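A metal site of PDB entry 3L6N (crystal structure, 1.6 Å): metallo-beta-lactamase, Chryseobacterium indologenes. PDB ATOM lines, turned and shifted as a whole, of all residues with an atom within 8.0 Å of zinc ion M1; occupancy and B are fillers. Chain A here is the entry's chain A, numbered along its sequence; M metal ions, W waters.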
ATOM      1  N   TRP A  49     -30.214   0.114 -17.507  1.00  0.00           N
ATOM      2  CA  TRP A  49     -28.891   0.654 -17.186  1.00  0.00           C
ATOM      3  C   TRP A  49     -28.392   0.154 -15.833  1.00  0.00           C
ATOM      4  O   TRP A  49     -27.211  -0.176 -15.679  1.00  0.00           O
ATOM      5  CB  TRP A  49     -28.904   2.182 -17.223  1.00  0.00           C
ATOM      6  CG  TRP A  49     -27.582   2.806 -17.636  1.00  0.00           C
ATOM      7  CD1 TRP A  49     -26.328   2.239 -17.572  1.00  0.00           C
ATOM      8  CD2 TRP A  49     -27.393   4.113 -18.191  1.00  0.00           C
ATOM      9  NE1 TRP A  49     -25.380   3.117 -18.048  1.00  0.00           N
ATOM     10  CE2 TRP A  49     -26.008   4.271 -18.433  1.00  0.00           C
ATOM     11  CE3 TRP A  49     -28.270   5.171 -18.484  1.00  0.00           C
ATOM     12  CZ2 TRP A  49     -25.474   5.447 -18.993  1.00  0.00           C
ATOM     13  CZ3 TRP A  49     -27.727   6.350 -19.059  1.00  0.00           C
ATOM     14  CH2 TRP A  49     -26.343   6.468 -19.289  1.00  0.00           C
ATOM     15  N   THR A  75     -26.850  -4.472 -28.260  1.00  0.00           N
ATOM     16  CA  THR A  75     -26.407  -3.684 -29.410  1.00  0.00           C
ATOM     17  C   THR A  75     -24.969  -3.156 -29.291  1.00  0.00           C
ATOM     18  O   THR A  75     -24.450  -2.551 -30.239  1.00  0.00           O
ATOM     19  CB  THR A  75     -27.390  -2.558 -29.825  1.00  0.00           C
ATOM     20  OG1 THR A  75     -27.450  -1.575 -28.787  1.00  0.00           O
ATOM     21  CG2 THR A  75     -28.781  -3.119 -30.102  1.00  0.00           C
ATOM     22  N   HIS A  76     -24.361  -3.355 -28.135  1.00  0.00           N
ATOM     23  CA  HIS A  76     -22.892  -3.358 -27.956  1.00  0.00           C
ATOM     24  C   HIS A  76     -22.554  -3.775 -26.519  1.00  0.00           C
ATOM     25  O   HIS A  76     -23.460  -4.179 -25.765  1.00  0.00           O
ATOM     26  CB  HIS A  76     -22.157  -2.069 -28.440  1.00  0.00           C
ATOM     27  CG  HIS A  76     -22.496  -0.798 -27.704  1.00  0.00           C
ATOM     28  ND1 HIS A  76     -23.618  -0.048 -27.991  1.00  0.00           N
ATOM     29  CD2 HIS A  76     -21.785  -0.096 -26.789  1.00  0.00           C
ATOM     30  CE1 HIS A  76     -23.623   1.032 -27.224  1.00  0.00           C
ATOM     31  NE2 HIS A  76     -22.524   1.029 -26.485  1.00  0.00           N
ATOM     32  N   SER A  77     -21.278  -3.700 -26.145  1.00  0.00           N
ATOM     33  CA  SER A  77     -20.824  -4.344 -24.901  1.00  0.00           C
ATOM     34  C   SER A  77     -21.035  -3.538 -23.630  1.00  0.00           C
ATOM     35  O   SER A  77     -20.859  -4.086 -22.541  1.00  0.00           O
ATOM     36  CB  SER A  77     -19.351  -4.710 -24.987  1.00  0.00           C
ATOM     37  OG  SER A  77     -18.538  -3.544 -24.886  1.00  0.00           O
ATOM     38  N   HIS A  78     -21.378  -2.267 -23.752  1.00  0.00           N
ATOM     39  CA  HIS A  78     -21.432  -1.367 -22.597  1.00  0.00           C
ATOM     40  C   HIS A  78     -22.559  -1.677 -21.621  1.00  0.00           C
ATOM     41  O   HIS A  78     -23.518  -2.388 -21.936  1.00  0.00           O
ATOM     42  CB  HIS A  78     -21.552   0.084 -23.066  1.00  0.00           C
ATOM     43  CG  HIS A  78     -20.284   0.637 -23.641  1.00  0.00           C
ATOM     44  ND1 HIS A  78     -20.263   1.765 -24.447  1.00  0.00           N
ATOM     45  CD2 HIS A  78     -18.997   0.253 -23.501  1.00  0.00           C
ATOM     46  CE1 HIS A  78     -19.009   2.039 -24.766  1.00  0.00           C
ATOM     47  NE2 HIS A  78     -18.227   1.127 -24.223  1.00  0.00           N
ATOM     48  N   ASP A  79     -22.425  -1.140 -20.414  1.00  0.00           N
ATOM     49  CA  ASP A  79     -23.370  -1.422 -19.309  1.00  0.00           C
ATOM     50  C   ASP A  79     -24.833  -1.111 -19.598  1.00  0.00           C
ATOM     51  O   ASP A  79     -25.728  -1.786 -19.071  1.00  0.00           O
ATOM     52  CB  ASP A  79     -22.981  -0.633 -18.065  1.00  0.00           C
ATOM     53  CG  ASP A  79     -21.681  -1.090 -17.432  1.00  0.00           C
ATOM     54  OD1 ASP A  79     -21.220  -0.370 -16.526  1.00  0.00           O
ATOM     55  OD2 ASP A  79     -21.124  -2.140 -17.807  1.00  0.00           O
ATOM     56  N   ASP A  80     -25.078  -0.086 -20.422  1.00  0.00           N
ATOM     57  CA  ASP A  80     -26.432   0.327 -20.793  1.00  0.00           C
ATOM     58  C   ASP A  80     -26.987  -0.483 -21.973  1.00  0.00           C
ATOM     59  O   ASP A  80     -28.074  -0.196 -22.460  1.00  0.00           O
ATOM     60  CB  ASP A  80     -26.487   1.843 -21.108  1.00  0.00           C
ATOM     61  CG  ASP A  80     -25.580   2.241 -22.253  1.00  0.00           C
ATOM     62  OD1 ASP A  80     -24.393   1.865 -22.259  1.00  0.00           O
ATOM     63  OD2 ASP A  80     -26.055   2.974 -23.164  1.00  0.00           O
ATOM     64  N   ARG A  81     -26.241  -1.507 -22.382  1.00  0.00           N
ATOM     65  CA  ARG A  81     -26.594  -2.285 -23.567  1.00  0.00           C
ATOM     66  C   ARG A  81     -26.615  -3.764 -23.207  1.00  0.00           C
ATOM     67  O   ARG A  81     -27.652  -4.283 -22.791  1.00  0.00           O
ATOM     68  CB  ARG A  81     -25.620  -1.966 -24.707  1.00  0.00           C
ATOM     69  CG  ARG A  81     -25.497  -0.472 -25.040  1.00  0.00           C
ATOM     70  CD  ARG A  81     -26.606   0.018 -25.955  1.00  0.00           C
ATOM     71  NE  ARG A  81     -27.869   0.252 -25.257  1.00  0.00           N
ATOM     72  CZ  ARG A  81     -28.892   0.911 -25.779  1.00  0.00           C
ATOM     73  NH1 ARG A  81     -28.811   1.386 -27.014  1.00  0.00           N
ATOM     74  NH2 ARG A  81     -30.008   1.072 -25.088  1.00  0.00           N
ATOM     75  N   HIS A 139     -19.755   4.988 -32.326  1.00  0.00           N
ATOM     76  CA  HIS A 139     -19.742   5.133 -30.880  1.00  0.00           C
ATOM     77  C   HIS A 139     -18.778   4.111 -30.246  1.00  0.00           C
ATOM     78  O   HIS A 139     -18.062   4.441 -29.314  1.00  0.00           O
ATOM     79  CB  HIS A 139     -21.154   4.961 -30.326  1.00  0.00           C
ATOM     80  CG  HIS A 139     -21.205   4.747 -28.840  1.00  0.00           C
ATOM     81  ND1 HIS A 139     -20.971   5.750 -27.925  1.00  0.00           N
ATOM     82  CD2 HIS A 139     -21.443   3.627 -28.121  1.00  0.00           C
ATOM     83  CE1 HIS A 139     -21.074   5.257 -26.701  1.00  0.00           C
ATOM     84  NE2 HIS A 139     -21.360   3.967 -26.795  1.00  0.00           N
ATOM     85  N   THR A 140     -18.821   2.875 -30.744  1.00  0.00           N
ATOM     86  CA  THR A 140     -17.820   1.858 -30.440  1.00  0.00           C
ATOM     87  C   THR A 140     -17.498   1.074 -31.712  1.00  0.00           C
ATOM     88  O   THR A 140     -18.128   1.281 -32.755  1.00  0.00           O
ATOM     89  CB  THR A 140     -18.341   0.855 -29.401  1.00  0.00           C
ATOM     90  OG1 THR A 140     -19.585   0.320 -29.872  1.00  0.00           O
ATOM     91  CG2 THR A 140     -18.522   1.509 -28.034  1.00  0.00           C
ATOM     92  N   ASP A 142     -18.028  -2.058 -32.073  1.00  0.00           N
ATOM     93  CA  ASP A 142     -18.969  -3.182 -32.162  1.00  0.00           C
ATOM     94  C   ASP A 142     -20.444  -2.762 -32.281  1.00  0.00           C
ATOM     95  O   ASP A 142     -21.330  -3.621 -32.333  1.00  0.00           O
ATOM     96  CB  ASP A 142     -18.794  -4.146 -30.972  1.00  0.00           C
ATOM     97  CG  ASP A 142     -19.168  -3.503 -29.625  1.00  0.00           C
ATOM     98  OD1 ASP A 142     -18.908  -2.295 -29.434  1.00  0.00           O
ATOM     99  OD2 ASP A 142     -19.707  -4.215 -28.741  1.00  0.00           O
ATOM    100  N   ASN A 143     -20.707  -1.469 -32.285  1.00  0.00           N
ATOM    101  CA  ASN A 143     -22.113  -1.034 -32.279  1.00  0.00           C
ATOM    102  C   ASN A 143     -22.907  -1.544 -33.482  1.00  0.00           C
ATOM    103  O   ASN A 143     -22.417  -1.510 -34.618  1.00  0.00           O
ATOM    104  CB  ASN A 143     -22.299   0.480 -32.059  1.00  0.00           C
ATOM    105  CG  ASN A 143     -21.486   1.369 -33.015  1.00  0.00           C
ATOM    106  OD1 ASN A 143     -21.239   2.519 -32.685  1.00  0.00           O
ATOM    107  ND2 ASN A 143     -21.134   0.868 -34.198  1.00  0.00           N
ATOM    108  N   GLY A 157     -29.479   2.825 -31.376  1.00  0.00           N
ATOM    109  CA  GLY A 157     -28.569   2.688 -30.251  1.00  0.00           C
ATOM    110  C   GLY A 157     -27.653   3.896 -30.137  1.00  0.00           C
ATOM    111  O   GLY A 157     -27.952   4.988 -30.647  1.00  0.00           O
ATOM    112  N   CYS A 158     -26.503   3.690 -29.530  1.00  0.00           N
ATOM    113  CA  CYS A 158     -25.671   4.802 -29.144  1.00  0.00           C
ATOM    114  C   CYS A 158     -24.831   5.330 -30.323  1.00  0.00           C
ATOM    115  O   CYS A 158     -24.164   6.355 -30.206  1.00  0.00           O
ATOM    116  CB  CYS A 158     -24.864   4.421 -27.902  1.00  0.00           C
ATOM    117  SG  CYS A 158     -25.954   3.606 -26.660  1.00  0.00           S
ATOM    118  N   LEU A 159     -24.916   4.639 -31.456  1.00  0.00           N
ATOM    119  CA  LEU A 159     -24.375   5.138 -32.727  1.00  0.00           C
ATOM    120  C   LEU A 159     -25.100   6.428 -33.136  1.00  0.00           C
ATOM    121  O   LEU A 159     -24.513   7.316 -33.755  1.00  0.00           O
ATOM    122  CB  LEU A 159     -24.564   4.064 -33.803  1.00  0.00           C
ATOM    123  CG  LEU A 159     -24.185   4.387 -35.258  1.00  0.00           C
ATOM    124  CD1 LEU A 159     -22.666   4.641 -35.372  1.00  0.00           C
ATOM    125  CD2 LEU A 159     -24.624   3.254 -36.159  1.00  0.00           C
ATOM    126  N   TYR A 170     -19.703   9.697 -24.179  1.00  0.00           N
ATOM    127  CA  TYR A 170     -18.527   8.872 -23.923  1.00  0.00           C
ATOM    128  C   TYR A 170     -17.870   8.418 -25.222  1.00  0.00           C
ATOM    129  O   TYR A 170     -18.443   7.619 -25.966  1.00  0.00           O
ATOM    130  CB  TYR A 170     -18.910   7.659 -23.066  1.00  0.00           C
ATOM    131  CG  TYR A 170     -17.765   6.734 -22.761  1.00  0.00           C
ATOM    132  CD1 TYR A 170     -16.767   7.084 -21.834  1.00  0.00           C
ATOM    133  CD2 TYR A 170     -17.657   5.493 -23.387  1.00  0.00           C
ATOM    134  CE1 TYR A 170     -15.712   6.216 -21.553  1.00  0.00           C
ATOM    135  CE2 TYR A 170     -16.602   4.629 -23.120  1.00  0.00           C
ATOM    136  CZ  TYR A 170     -15.634   4.997 -22.200  1.00  0.00           C
ATOM    137  OH  TYR A 170     -14.590   4.128 -21.941  1.00  0.00           O
ATOM    138  N   GLU A 173     -13.889   4.991 -26.431  1.00  0.00           N
ATOM    139  CA  GLU A 173     -13.834   3.755 -27.229  1.00  0.00           C
ATOM    140  C   GLU A 173     -14.468   3.945 -28.598  1.00  0.00           C
ATOM    141  O   GLU A 173     -14.764   2.985 -29.300  1.00  0.00           O
ATOM    142  CB  GLU A 173     -14.481   2.601 -26.450  1.00  0.00           C
ATOM    143  CG  GLU A 173     -13.770   2.361 -25.106  1.00  0.00           C
ATOM    144  CD  GLU A 173     -14.389   1.274 -24.252  1.00  0.00           C
ATOM    145  OE1 GLU A 173     -15.481   0.768 -24.592  1.00  0.00           O
ATOM    146  OE2 GLU A 173     -13.758   0.913 -23.236  1.00  0.00           O
ATOM    147  N   HIS A 200     -29.457   7.414 -26.148  1.00  0.00           N
ATOM    148  CA  HIS A 200     -29.582   8.222 -24.933  1.00  0.00           C
ATOM    149  C   HIS A 200     -30.416   9.469 -25.178  1.00  0.00           C
ATOM    150  O   HIS A 200     -30.541   9.918 -26.318  1.00  0.00           O
ATOM    151  CB  HIS A 200     -28.202   8.641 -24.444  1.00  0.00           C
ATOM    152  CG  HIS A 200     -27.321   7.490 -24.052  1.00  0.00           C
ATOM    153  ND1 HIS A 200     -27.354   6.925 -22.793  1.00  0.00           N
ATOM    154  CD2 HIS A 200     -26.380   6.816 -24.753  1.00  0.00           C
ATOM    155  CE1 HIS A 200     -26.462   5.946 -22.744  1.00  0.00           C
ATOM    156  NE2 HIS A 200     -25.869   5.857 -23.912  1.00  0.00           N
HETATM  157 ZN    ZN M   1     -21.816   2.650 -25.361  1.00  0.00          ZN
HETATM  158 ZN    ZN M   2     -25.115   4.012 -24.659  1.00  0.00          ZN
HETATM  159  O   HOH W   1     -23.241   3.233 -24.221  1.00  0.00           O
HETATM  160  O   HOH W   2     -20.790   4.301 -23.624  1.00  0.00           O
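N of His 139 sits at hydrogen-bond distance from OD1 of Asn 143 (2.9 Å).
NE2 of His 78 is in hydrogen-bond range of OE1 of Glu 173, 2.8 Å away.
The nearest printed residue that does not touch zinc ion M1 is Asp 80 (4.1 Å).
Zinc ion M1 is bound by water W1, NE2 of His 139, ND1 of His 78 and NE2 of His 76.
Zinc ion M1 has four donor atoms within binding distance.
Slightly farther from zinc ion M1 lies water W2 (2.6 Å).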
